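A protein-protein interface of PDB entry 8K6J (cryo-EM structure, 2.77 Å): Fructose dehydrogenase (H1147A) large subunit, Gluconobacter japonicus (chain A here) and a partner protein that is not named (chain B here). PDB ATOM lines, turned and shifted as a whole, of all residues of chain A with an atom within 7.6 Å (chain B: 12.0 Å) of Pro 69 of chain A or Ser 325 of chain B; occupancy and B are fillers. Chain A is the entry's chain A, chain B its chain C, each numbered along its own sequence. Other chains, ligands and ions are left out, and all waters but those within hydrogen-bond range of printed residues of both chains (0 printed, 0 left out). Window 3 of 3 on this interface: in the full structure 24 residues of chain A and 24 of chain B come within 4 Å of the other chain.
O of Arg 323 of chain B lies within hydrogen-bond range of NE2 of Gln 46 of chain A (3.3 Å). The side-chain amide oxygen (OE1) of Gln 46 of chain A sits at hydrogen-bond distance from the side-chain hydroxyl (OG1) of Thr 332 of chain B.
NH2 of Arg 42 of chain A is in hydrogen-bond range of O of Pro 69 of chain A, 3.1 Å away. The guanidinium group of Arg 42 of chain A is in hydrogen-bond range of the backbone carbonyl oxygen of Lys 102 of chain A (2.5 Å). The side-chain amide nitrogen (ND2) of Asn 50 of chain A lies within hydrogen-bond range of the backbone carbonyl oxygen (O) of Pro 67 of chain A. The backbone carbonyl oxygen (O) of Pro 69 of chain A sits at hydrogen-bond distance from a ring nitrogen (NE2) of His 76 of chain A. NE of Arg 324 of chain B lies within hydrogen-bond range of O of Asn 321 of chain B (3.4 Å). OG1 of Thr 330 of chain B is in hydrogen-bond range of O of Thr 328 of chain B, at 3.3 Å.
Among the printed residues, merely in contact across the chains: Arg 42 of chain A with Ser 327 of chain B (3.7 Å), Arg 42 of chain A with Thr 328 of chain B (3.5 Å), Gln 46 of chain A with Asn 326 of chain B (3.1 Å), Gln 46 of chain A with Ser 327 of chain B (3.6 Å), Gln 46 of chain A with Thr 328 of chain B (3.998 Å), Gln 46 of chain A with Leu 329 of chain B (3.2 Å), Asn 50 of chain A with Arg 323 of chain B (3.7 Å), Asn 50 of chain A with Arg 324 of chain B (3.9 Å), Pro 69 of chain A with Ser 325 of chain B (3.5 Å), Pro 69 of chain A with Asn 326 of chain B (3.8 Å) and Pro 69 of chain A with Ser 327 of chain B (3.7 Å).
Printed residues of chain B within 4 Å of Arg 42 of chain A: Ser 327 and Thr 328. No residue of chain B comes within 4 Å of Pro 67 of chain A. Printed residues of chain B within 4 Å of Pro 69 of chain A: Ser 325 (3.5 Å), Asn 326 (3.8 Å) and Ser 327 (3.7 Å). Val 71 of chain A touches none of the printed residues of chain B. Ser 322 of chain B touches none of the printed residues of chain A. Of the printed residues of chain A, Arg 324 of chain B touches Asn 50. Of the printed residues of chain A, Ser 325 of chain B touches Pro 69. Printed residues of chain A within 4 Å of Asn 326 of chain B: Gln 46 (3.1 Å) and Pro 69 (3.8 Å). Of the printed residues of chain A, Ser 327 of chain B touches Arg 42 (3.7 Å), Gln 46 (3.6 Å) and Pro 69 (3.7 Å). Of the printed residues of chain A, Thr 328 of chain B touches Arg 42 and Gln 46.
Of the 20 printed residues of chain A, 4 touch a printed residue of chain B. Printed residues of chain A that touch a printed residue of chain B: Arg 42, Gln 46, Asn 50 and Pro 69. Of the 16 printed residues of chain B, 8 touch a printed residue of chain A. Hydrophobic or aromatic side chains of chain B that line the printed part of chain A: Leu 329. Among the printed residues, 13 pairs touch across the chains. Among the printed residues, no Asp or Glu carboxylate lies within 4 Å of a Lys or Arg side-chain nitrogen of the other chain.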
ATOM      1  N   GLY A  39      11.558 -29.534 -27.007  1.00  0.00           N
ATOM      2  CA  GLY A  39      12.619 -28.582 -26.792  1.00  0.00           C
ATOM      3  C   GLY A  39      12.164 -27.382 -25.989  1.00  0.00           C
ATOM      4  O   GLY A  39      10.993 -27.257 -25.624  1.00  0.00           O
ATOM      5  N   PRO A  40      13.089 -26.477 -25.697  1.00  0.00           N
ATOM      6  CA  PRO A  40      12.754 -25.279 -24.930  1.00  0.00           C
ATOM      7  C   PRO A  40      12.358 -24.120 -25.838  1.00  0.00           C
ATOM      8  O   PRO A  40      12.470 -24.183 -27.062  1.00  0.00           O
ATOM      9  CB  PRO A  40      14.066 -24.972 -24.204  1.00  0.00           C
ATOM     10  CG  PRO A  40      15.115 -25.424 -25.170  1.00  0.00           C
ATOM     11  CD  PRO A  40      14.530 -26.556 -25.985  1.00  0.00           C
ATOM     12  N   ARG A  42      13.035 -20.659 -27.546  1.00  0.00           N
ATOM     13  CA  ARG A  42      14.258 -20.081 -28.080  1.00  0.00           C
ATOM     14  C   ARG A  42      14.008 -18.643 -28.499  1.00  0.00           C
ATOM     15  O   ARG A  42      12.933 -18.310 -29.002  1.00  0.00           O
ATOM     16  CB  ARG A  42      14.782 -20.886 -29.271  1.00  0.00           C
ATOM     17  CG  ARG A  42      14.853 -22.378 -29.028  1.00  0.00           C
ATOM     18  CD  ARG A  42      15.934 -23.013 -29.872  1.00  0.00           C
ATOM     19  NE  ARG A  42      16.040 -24.447 -29.636  1.00  0.00           N
ATOM     20  CZ  ARG A  42      16.911 -25.007 -28.809  1.00  0.00           C
ATOM     21  NH1 ARG A  42      17.764 -24.279 -28.109  1.00  0.00           N
ATOM     22  NH2 ARG A  42      16.928 -26.329 -28.683  1.00  0.00           N
ATOM     23  N   GLN A  46      19.238 -14.261 -29.126  1.00  0.00           N
ATOM     24  CA  GLN A  46      20.240 -15.078 -28.452  1.00  0.00           C
ATOM     25  C   GLN A  46      20.888 -16.060 -29.418  1.00  0.00           C
ATOM     26  O   GLN A  46      22.092 -16.319 -29.330  1.00  0.00           O
ATOM     27  CB  GLN A  46      19.618 -15.814 -27.272  1.00  0.00           C
ATOM     28  CG  GLN A  46      20.619 -16.605 -26.463  1.00  0.00           C
ATOM     29  CD  GLN A  46      21.849 -15.802 -26.102  1.00  0.00           C
ATOM     30  OE1 GLN A  46      21.756 -14.743 -25.491  1.00  0.00           O
ATOM     31  NE2 GLN A  46      23.014 -16.309 -26.479  1.00  0.00           N
ATOM     32  N   ILE A  47      20.109 -16.619 -30.344  1.00  0.00           N
ATOM     33  CA  ILE A  47      20.685 -17.497 -31.358  1.00  0.00           C
ATOM     34  C   ILE A  47      21.639 -16.719 -32.252  1.00  0.00           C
ATOM     35  O   ILE A  47      22.691 -17.228 -32.656  1.00  0.00           O
ATOM     36  CB  ILE A  47      19.574 -18.175 -32.179  1.00  0.00           C
ATOM     37  CG1 ILE A  47      18.603 -18.918 -31.262  1.00  0.00           C
ATOM     38  CG2 ILE A  47      20.175 -19.115 -33.200  1.00  0.00           C
ATOM     39  CD1 ILE A  47      19.275 -19.811 -30.253  1.00  0.00           C
ATOM     40  N   ASN A  50      24.788 -16.315 -30.336  1.00  0.00           N
ATOM     41  CA  ASN A  50      25.513 -17.581 -30.311  1.00  0.00           C
ATOM     42  C   ASN A  50      26.234 -17.826 -31.628  1.00  0.00           C
ATOM     43  O   ASN A  50      27.378 -18.293 -31.641  1.00  0.00           O
ATOM     44  CB  ASN A  50      24.557 -18.731 -30.011  1.00  0.00           C
ATOM     45  CG  ASN A  50      23.975 -18.658 -28.620  1.00  0.00           C
ATOM     46  OD1 ASN A  50      24.247 -17.723 -27.872  1.00  0.00           O
ATOM     47  ND2 ASN A  50      23.168 -19.646 -28.265  1.00  0.00           N
ATOM     48  N   ALA A  65      23.804 -25.986 -36.244  1.00  0.00           N
ATOM     49  CA  ALA A  65      23.227 -26.501 -35.012  1.00  0.00           C
ATOM     50  C   ALA A  65      23.888 -25.974 -33.751  1.00  0.00           C
ATOM     51  O   ALA A  65      23.231 -25.926 -32.711  1.00  0.00           O
ATOM     52  CB  ALA A  65      23.289 -28.034 -34.997  1.00  0.00           C
ATOM     53  N   THR A  66      25.162 -25.592 -33.809  1.00  0.00           N
ATOM     54  CA  THR A  66      25.827 -25.052 -32.627  1.00  0.00           C
ATOM     55  C   THR A  66      25.129 -23.830 -32.035  1.00  0.00           C
ATOM     56  O   THR A  66      25.058 -23.742 -30.797  1.00  0.00           O
ATOM     57  CB  THR A  66      27.290 -24.739 -32.953  1.00  0.00           C
ATOM     58  OG1 THR A  66      27.930 -25.919 -33.451  1.00  0.00           O
ATOM     59  CG2 THR A  66      28.024 -24.269 -31.713  1.00  0.00           C
ATOM     60  N   PRO A  67      24.617 -22.869 -32.815  1.00  0.00           N
ATOM     61  CA  PRO A  67      23.896 -21.751 -32.188  1.00  0.00           C
ATOM     62  C   PRO A  67      22.720 -22.186 -31.334  1.00  0.00           C
ATOM     63  O   PRO A  67      22.378 -21.490 -30.371  1.00  0.00           O
ATOM     64  CB  PRO A  67      23.437 -20.917 -33.390  1.00  0.00           C
ATOM     65  CG  PRO A  67      24.435 -21.200 -34.428  1.00  0.00           C
ATOM     66  CD  PRO A  67      24.791 -22.641 -34.261  1.00  0.00           C
ATOM     67  N   TYR A  68      22.091 -23.315 -31.652  1.00  0.00           N
ATOM     68  CA  TYR A  68      20.968 -23.801 -30.869  1.00  0.00           C
ATOM     69  C   TYR A  68      21.469 -24.825 -29.867  1.00  0.00           C
ATOM     70  O   TYR A  68      21.874 -25.925 -30.273  1.00  0.00           O
ATOM     71  CB  TYR A  68      19.908 -24.417 -31.777  1.00  0.00           C
ATOM     72  CG  TYR A  68      19.439 -23.490 -32.867  1.00  0.00           C
ATOM     73  CD1 TYR A  68      20.087 -23.446 -34.090  1.00  0.00           C
ATOM     74  CD2 TYR A  68      18.351 -22.656 -32.673  1.00  0.00           C
ATOM     75  CE1 TYR A  68      19.665 -22.600 -35.085  1.00  0.00           C
ATOM     76  CE2 TYR A  68      17.922 -21.807 -33.664  1.00  0.00           C
ATOM     77  CZ  TYR A  68      18.584 -21.784 -34.868  1.00  0.00           C
ATOM     78  OH  TYR A  68      18.159 -20.939 -35.862  1.00  0.00           O
ATOM     79  N   PRO A  69      21.468 -24.522 -28.572  1.00  0.00           N
ATOM     80  CA  PRO A  69      21.961 -25.490 -27.587  1.00  0.00           C
ATOM     81  C   PRO A  69      21.112 -26.752 -27.578  1.00  0.00           C
ATOM     82  O   PRO A  69      19.887 -26.700 -27.701  1.00  0.00           O
ATOM     83  CB  PRO A  69      21.857 -24.733 -26.260  1.00  0.00           C
ATOM     84  CG  PRO A  69      21.687 -23.299 -26.635  1.00  0.00           C
ATOM     85  CD  PRO A  69      20.995 -23.282 -27.944  1.00  0.00           C
ATOM     86  N   SER A  70      21.777 -27.891 -27.418  1.00  0.00           N
ATOM     87  CA  SER A  70      21.111 -29.188 -27.410  1.00  0.00           C
ATOM     88  C   SER A  70      20.770 -29.548 -25.970  1.00  0.00           C
ATOM     89  O   SER A  70      21.658 -29.879 -25.180  1.00  0.00           O
ATOM     90  CB  SER A  70      21.996 -30.254 -28.049  1.00  0.00           C
ATOM     91  OG  SER A  70      21.346 -31.511 -28.068  1.00  0.00           O
ATOM     92  N   VAL A  71      19.491 -29.478 -25.630  1.00  0.00           N
ATOM     93  CA  VAL A  71      19.066 -29.792 -24.263  1.00  0.00           C
ATOM     94  C   VAL A  71      19.190 -31.293 -24.031  1.00  0.00           C
ATOM     95  O   VAL A  71      18.839 -32.083 -24.924  1.00  0.00           O
ATOM     96  CB  VAL A  71      17.636 -29.308 -24.029  1.00  0.00           C
ATOM     97  CG1 VAL A  71      17.625 -27.805 -23.844  1.00  0.00           C
ATOM     98  CG2 VAL A  71      16.751 -29.698 -25.196  1.00  0.00           C
ATOM     99  N   PRO A  72      19.692 -31.732 -22.874  1.00  0.00           N
ATOM    100  CA  PRO A  72      19.918 -33.172 -22.673  1.00  0.00           C
ATOM    101  C   PRO A  72      18.661 -34.019 -22.754  1.00  0.00           C
ATOM    102  O   PRO A  72      18.730 -35.158 -23.230  1.00  0.00           O
ATOM    103  CB  PRO A  72      20.549 -33.233 -21.276  1.00  0.00           C
ATOM    104  CG  PRO A  72      20.148 -31.962 -20.615  1.00  0.00           C
ATOM    105  CD  PRO A  72      20.084 -30.938 -21.699  1.00  0.00           C
ATOM    106  N   ALA A  74      15.885 -33.510 -24.569  1.00  0.00           N
ATOM    107  CA  ALA A  74      15.422 -33.574 -25.954  1.00  0.00           C
ATOM    108  C   ALA A  74      16.554 -33.135 -26.871  1.00  0.00           C
ATOM    109  O   ALA A  74      16.518 -32.044 -27.450  1.00  0.00           O
ATOM    110  CB  ALA A  74      14.181 -32.707 -26.159  1.00  0.00           C
ATOM    111  N   PRO A  75      17.582 -33.965 -27.022  1.00  0.00           N
ATOM    112  CA  PRO A  75      18.730 -33.565 -27.836  1.00  0.00           C
ATOM    113  C   PRO A  75      18.386 -33.528 -29.313  1.00  0.00           C
ATOM    114  O   PRO A  75      17.488 -34.228 -29.785  1.00  0.00           O
ATOM    115  CB  PRO A  75      19.767 -34.651 -27.537  1.00  0.00           C
ATOM    116  CG  PRO A  75      18.955 -35.845 -27.204  1.00  0.00           C
ATOM    117  CD  PRO A  75      17.697 -35.352 -26.545  1.00  0.00           C
ATOM    118  N   HIS A  76      19.114 -32.692 -30.046  1.00  0.00           N
ATOM    119  CA  HIS A  76      19.021 -32.641 -31.494  1.00  0.00           C
ATOM    120  C   HIS A  76      20.410 -32.831 -32.083  1.00  0.00           C
ATOM    121  O   HIS A  76      21.422 -32.760 -31.382  1.00  0.00           O
ATOM    122  CB  HIS A  76      18.388 -31.330 -31.980  1.00  0.00           C
ATOM    123  CG  HIS A  76      19.104 -30.098 -31.522  1.00  0.00           C
ATOM    124  ND1 HIS A  76      20.329 -29.718 -32.024  1.00  0.00           N
ATOM    125  CD2 HIS A  76      18.752 -29.145 -30.628  1.00  0.00           C
ATOM    126  CE1 HIS A  76      20.708 -28.591 -31.449  1.00  0.00           C
ATOM    127  NE2 HIS A  76      19.769 -28.222 -30.597  1.00  0.00           N
ATOM    128  N   ASN A  78      23.935 -32.506 -33.796  1.00  0.00           N
ATOM    129  CA  ASN A  78      24.988 -31.492 -33.830  1.00  0.00           C
ATOM    130  C   ASN A  78      26.234 -32.191 -34.363  1.00  0.00           C
ATOM    131  O   ASN A  78      26.885 -32.938 -33.629  1.00  0.00           O
ATOM    132  CB  ASN A  78      25.222 -30.893 -32.453  1.00  0.00           C
ATOM    133  CG  ASN A  78      25.986 -29.594 -32.507  1.00  0.00           C
ATOM    134  OD1 ASN A  78      26.989 -29.479 -33.206  1.00  0.00           O
ATOM    135  ND2 ASN A  78      25.515 -28.601 -31.764  1.00  0.00           N
ATOM    136  N   ILE A 101      16.335 -29.261 -35.230  1.00  0.00           N
ATOM    137  CA  ILE A 101      16.389 -28.379 -34.073  1.00  0.00           C
ATOM    138  C   ILE A 101      15.138 -28.623 -33.247  1.00  0.00           C
ATOM    139  O   ILE A 101      14.028 -28.640 -33.787  1.00  0.00           O
ATOM    140  CB  ILE A 101      16.493 -26.898 -34.480  1.00  0.00           C
ATOM    141  CG1 ILE A 101      17.762 -26.659 -35.292  1.00  0.00           C
ATOM    142  CG2 ILE A 101      16.482 -26.010 -33.255  1.00  0.00           C
ATOM    143  CD1 ILE A 101      19.026 -26.889 -34.519  1.00  0.00           C
ATOM    144  N   LYS A 102      15.316 -28.819 -31.946  1.00  0.00           N
ATOM    145  CA  LYS A 102      14.210 -29.084 -31.040  1.00  0.00           C
ATOM    146  C   LYS A 102      13.930 -27.840 -30.212  1.00  0.00           C
ATOM    147  O   LYS A 102      14.844 -27.260 -29.620  1.00  0.00           O
ATOM    148  CB  LYS A 102      14.517 -30.280 -30.139  1.00  0.00           C
ATOM    149  CG  LYS A 102      14.372 -31.608 -30.854  1.00  0.00           C
ATOM    150  CD  LYS A 102      14.353 -32.765 -29.886  1.00  0.00           C
ATOM    151  CE  LYS A 102      14.339 -34.085 -30.625  1.00  0.00           C
ATOM    152  NZ  LYS A 102      13.768 -35.174 -29.790  1.00  0.00           N
ATOM    153  N   VAL B 317      32.902  -8.462 -27.489  1.00  0.00           N
ATOM    154  CA  VAL B 317      32.581  -9.770 -28.048  1.00  0.00           C
ATOM    155  C   VAL B 317      33.047 -10.878 -27.115  1.00  0.00           C
ATOM    156  O   VAL B 317      32.392 -11.919 -26.988  1.00  0.00           O
ATOM    157  CB  VAL B 317      33.194  -9.917 -29.451  1.00  0.00           C
ATOM    158  CG1 VAL B 317      32.695 -11.183 -30.117  1.00  0.00           C
ATOM    159  CG2 VAL B 317      32.869  -8.703 -30.297  1.00  0.00           C
ATOM    160  N   ALA B 318      34.185 -10.672 -26.448  1.00  0.00           N
ATOM    161  CA  ALA B 318      34.754 -11.714 -25.599  1.00  0.00           C
ATOM    162  C   ALA B 318      33.829 -12.058 -24.441  1.00  0.00           C
ATOM    163  O   ALA B 318      33.703 -13.229 -24.066  1.00  0.00           O
ATOM    164  CB  ALA B 318      36.121 -11.274 -25.079  1.00  0.00           C
ATOM    165  N   ASN B 319      33.176 -11.054 -23.853  1.00  0.00           N
ATOM    166  CA  ASN B 319      32.287 -11.306 -22.727  1.00  0.00           C
ATOM    167  C   ASN B 319      31.079 -12.147 -23.114  1.00  0.00           C
ATOM    168  O   ASN B 319      30.462 -12.759 -22.238  1.00  0.00           O
ATOM    169  CB  ASN B 319      31.820  -9.985 -22.118  1.00  0.00           C
ATOM    170  CG  ASN B 319      32.947  -9.214 -21.469  1.00  0.00           C
ATOM    171  OD1 ASN B 319      34.090  -9.667 -21.443  1.00  0.00           O
ATOM    172  ND2 ASN B 319      32.631  -8.040 -20.939  1.00  0.00           N
ATOM    173  N   ALA B 320      30.728 -12.192 -24.398  1.00  0.00           N
ATOM    174  CA  ALA B 320      29.566 -12.947 -24.843  1.00  0.00           C
ATOM    175  C   ALA B 320      29.830 -14.441 -24.950  1.00  0.00           C
ATOM    176  O   ALA B 320      28.880 -15.206 -25.146  1.00  0.00           O
ATOM    177  CB  ALA B 320      29.082 -12.421 -26.194  1.00  0.00           C
ATOM    178  N   ASN B 321      31.087 -14.872 -24.830  1.00  0.00           N
ATOM    179  CA  ASN B 321      31.400 -16.290 -24.961  1.00  0.00           C
ATOM    180  C   ASN B 321      30.756 -17.105 -23.848  1.00  0.00           C
ATOM    181  O   ASN B 321      30.273 -18.218 -24.084  1.00  0.00           O
ATOM    182  CB  ASN B 321      32.913 -16.492 -24.966  1.00  0.00           C
ATOM    183  CG  ASN B 321      33.532 -16.175 -26.304  1.00  0.00           C
ATOM    184  OD1 ASN B 321      33.146 -16.736 -27.325  1.00  0.00           O
ATOM    185  ND2 ASN B 321      34.495 -15.266 -26.310  1.00  0.00           N
ATOM    186  N   SER B 322      30.741 -16.569 -22.627  1.00  0.00           N
ATOM    187  CA  SER B 322      30.130 -17.277 -21.511  1.00  0.00           C
ATOM    188  C   SER B 322      28.630 -17.457 -21.690  1.00  0.00           C
ATOM    189  O   SER B 322      28.049 -18.350 -21.066  1.00  0.00           O
ATOM    190  CB  SER B 322      30.406 -16.535 -20.206  1.00  0.00           C
ATOM    191  OG  SER B 322      29.786 -15.262 -20.209  1.00  0.00           O
ATOM    192  N   ARG B 323      27.997 -16.642 -22.527  1.00  0.00           N
ATOM    193  CA  ARG B 323      26.558 -16.702 -22.736  1.00  0.00           C
ATOM    194  C   ARG B 323      26.165 -17.626 -23.877  1.00  0.00           C
ATOM    195  O   ARG B 323      24.993 -17.652 -24.260  1.00  0.00           O
ATOM    196  CB  ARG B 323      26.004 -15.300 -22.990  1.00  0.00           C
ATOM    197  CG  ARG B 323      25.633 -14.554 -21.726  1.00  0.00           C
ATOM    198  CD  ARG B 323      24.890 -13.275 -22.044  1.00  0.00           C
ATOM    199  NE  ARG B 323      25.496 -12.555 -23.156  1.00  0.00           N
ATOM    200  CZ  ARG B 323      26.437 -11.631 -23.024  1.00  0.00           C
ATOM    201  NH1 ARG B 323      26.917 -11.300 -21.838  1.00  0.00           N
ATOM    202  NH2 ARG B 323      26.908 -11.027 -24.109  1.00  0.00           N
ATOM    203  N   ARG B 324      27.114 -18.361 -24.448  1.00  0.00           N
ATOM    204  CA  ARG B 324      26.759 -19.387 -25.411  1.00  0.00           C
ATOM    205  C   ARG B 324      26.130 -20.576 -24.692  1.00  0.00           C
ATOM    206  O   ARG B 324      26.262 -20.739 -23.476  1.00  0.00           O
ATOM    207  CB  ARG B 324      27.985 -19.827 -26.206  1.00  0.00           C
ATOM    208  CG  ARG B 324      28.588 -18.723 -27.046  1.00  0.00           C
ATOM    209  CD  ARG B 324      29.753 -19.231 -27.863  1.00  0.00           C
ATOM    210  NE  ARG B 324      30.796 -19.796 -27.017  1.00  0.00           N
ATOM    211  CZ  ARG B 324      32.019 -20.086 -27.433  1.00  0.00           C
ATOM    212  NH1 ARG B 324      32.394 -19.868 -28.681  1.00  0.00           N
ATOM    213  NH2 ARG B 324      32.888 -20.610 -26.574  1.00  0.00           N
ATOM    214  N   SER B 325      25.428 -21.406 -25.460  1.00  0.00           N
ATOM    215  CA  SER B 325      24.639 -22.508 -24.908  1.00  0.00           C
ATOM    216  C   SER B 325      23.614 -22.001 -23.901  1.00  0.00           C
ATOM    217  O   SER B 325      23.270 -22.695 -22.941  1.00  0.00           O
ATOM    218  CB  SER B 325      25.532 -23.574 -24.268  1.00  0.00           C
ATOM    219  OG  SER B 325      25.869 -23.211 -22.941  1.00  0.00           O
ATOM    220  N   ASN B 326      23.122 -20.782 -24.116  1.00  0.00           N
ATOM    221  CA  ASN B 326      22.245 -20.094 -23.175  1.00  0.00           C
ATOM    222  C   ASN B 326      21.081 -19.458 -23.936  1.00  0.00           C
ATOM    223  O   ASN B 326      20.805 -18.267 -23.806  1.00  0.00           O
ATOM    224  CB  ASN B 326      23.030 -19.056 -22.376  1.00  0.00           C
ATOM    225  CG  ASN B 326      22.203 -18.396 -21.297  1.00  0.00           C
ATOM    226  OD1 ASN B 326      22.534 -17.310 -20.826  1.00  0.00           O
ATOM    227  ND2 ASN B 326      21.122 -19.050 -20.892  1.00  0.00           N
ATOM    228  N   SER B 327      20.412 -20.261 -24.765  1.00  0.00           N
ATOM    229  CA  SER B 327      19.260 -19.795 -25.532  1.00  0.00           C
ATOM    230  C   SER B 327      18.210 -19.175 -24.621  1.00  0.00           C
ATOM    231  O   SER B 327      18.228 -19.383 -23.405  1.00  0.00           O
ATOM    232  CB  SER B 327      18.646 -20.958 -26.312  1.00  0.00           C
ATOM    233  OG  SER B 327      17.539 -21.500 -25.617  1.00  0.00           O
ATOM    234  N   THR B 328      17.281 -18.421 -25.222  1.00  0.00           N
ATOM    235  CA  THR B 328      16.269 -17.685 -24.470  1.00  0.00           C
ATOM    236  C   THR B 328      16.986 -16.689 -23.558  1.00  0.00           C
ATOM    237  O   THR B 328      17.208 -16.951 -22.372  1.00  0.00           O
ATOM    238  CB  THR B 328      15.331 -18.643 -23.715  1.00  0.00           C
ATOM    239  OG1 THR B 328      14.355 -19.143 -24.633  1.00  0.00           O
ATOM    240  CG2 THR B 328      14.543 -17.922 -22.627  1.00  0.00           C
ATOM    241  N   LEU B 329      17.463 -15.588 -24.141  1.00  0.00           N
ATOM    242  CA  LEU B 329      18.395 -14.690 -23.459  1.00  0.00           C
ATOM    243  C   LEU B 329      17.687 -14.025 -22.279  1.00  0.00           C
ATOM    244  O   LEU B 329      16.978 -13.023 -22.396  1.00  0.00           O
ATOM    245  CB  LEU B 329      18.974 -13.661 -24.432  1.00  0.00           C
ATOM    246  CG  LEU B 329      18.230 -12.443 -25.009  1.00  0.00           C
ATOM    247  CD1 LEU B 329      19.089 -11.724 -26.033  1.00  0.00           C
ATOM    248  CD2 LEU B 329      16.888 -12.807 -25.616  1.00  0.00           C
ATOM    249  N   THR B 330      17.873 -14.629 -21.109  1.00  0.00           N
ATOM    250  CA  THR B 330      17.450 -14.040 -19.848  1.00  0.00           C
ATOM    251  C   THR B 330      18.621 -13.615 -18.981  1.00  0.00           C
ATOM    252  O   THR B 330      18.467 -12.722 -18.142  1.00  0.00           O
ATOM    253  CB  THR B 330      16.578 -15.025 -19.065  1.00  0.00           C
ATOM    254  OG1 THR B 330      17.183 -16.322 -19.090  1.00  0.00           O
ATOM    255  CG2 THR B 330      15.191 -15.111 -19.681  1.00  0.00           C
ATOM    256  N   LYS B 331      19.785 -14.232 -19.165  1.00  0.00           N
ATOM    257  CA  LYS B 331      21.001 -13.845 -18.466  1.00  0.00           C
ATOM    258  C   LYS B 331      21.752 -12.729 -19.174  1.00  0.00           C
ATOM    259  O   LYS B 331      22.780 -12.273 -18.666  1.00  0.00           O
ATOM    260  CB  LYS B 331      21.920 -15.056 -18.295  1.00  0.00           C
ATOM    261  CG  LYS B 331      21.193 -16.331 -17.907  1.00  0.00           C
ATOM    262  CD  LYS B 331      21.936 -17.075 -16.811  1.00  0.00           C
ATOM    263  CE  LYS B 331      21.854 -18.577 -17.012  1.00  0.00           C
ATOM    264  NZ  LYS B 331      20.543 -18.989 -17.582  1.00  0.00           N
ATOM    265  N   THR B 332      21.271 -12.283 -20.333  1.00  0.00           N
ATOM    266  CA  THR B 332      21.891 -11.175 -21.057  1.00  0.00           C
ATOM    267  C   THR B 332      21.324  -9.855 -20.536  1.00  0.00           C
ATOM    268  O   THR B 332      20.528  -9.174 -21.182  1.00  0.00           O
ATOM    269  CB  THR B 332      21.669 -11.326 -22.555  1.00  0.00           C
ATOM    270  OG1 THR B 332      21.784 -12.707 -22.917  1.00  0.00           O
ATOM    271  CG2 THR B 332      22.699 -10.519 -23.326  1.00  0.00           C
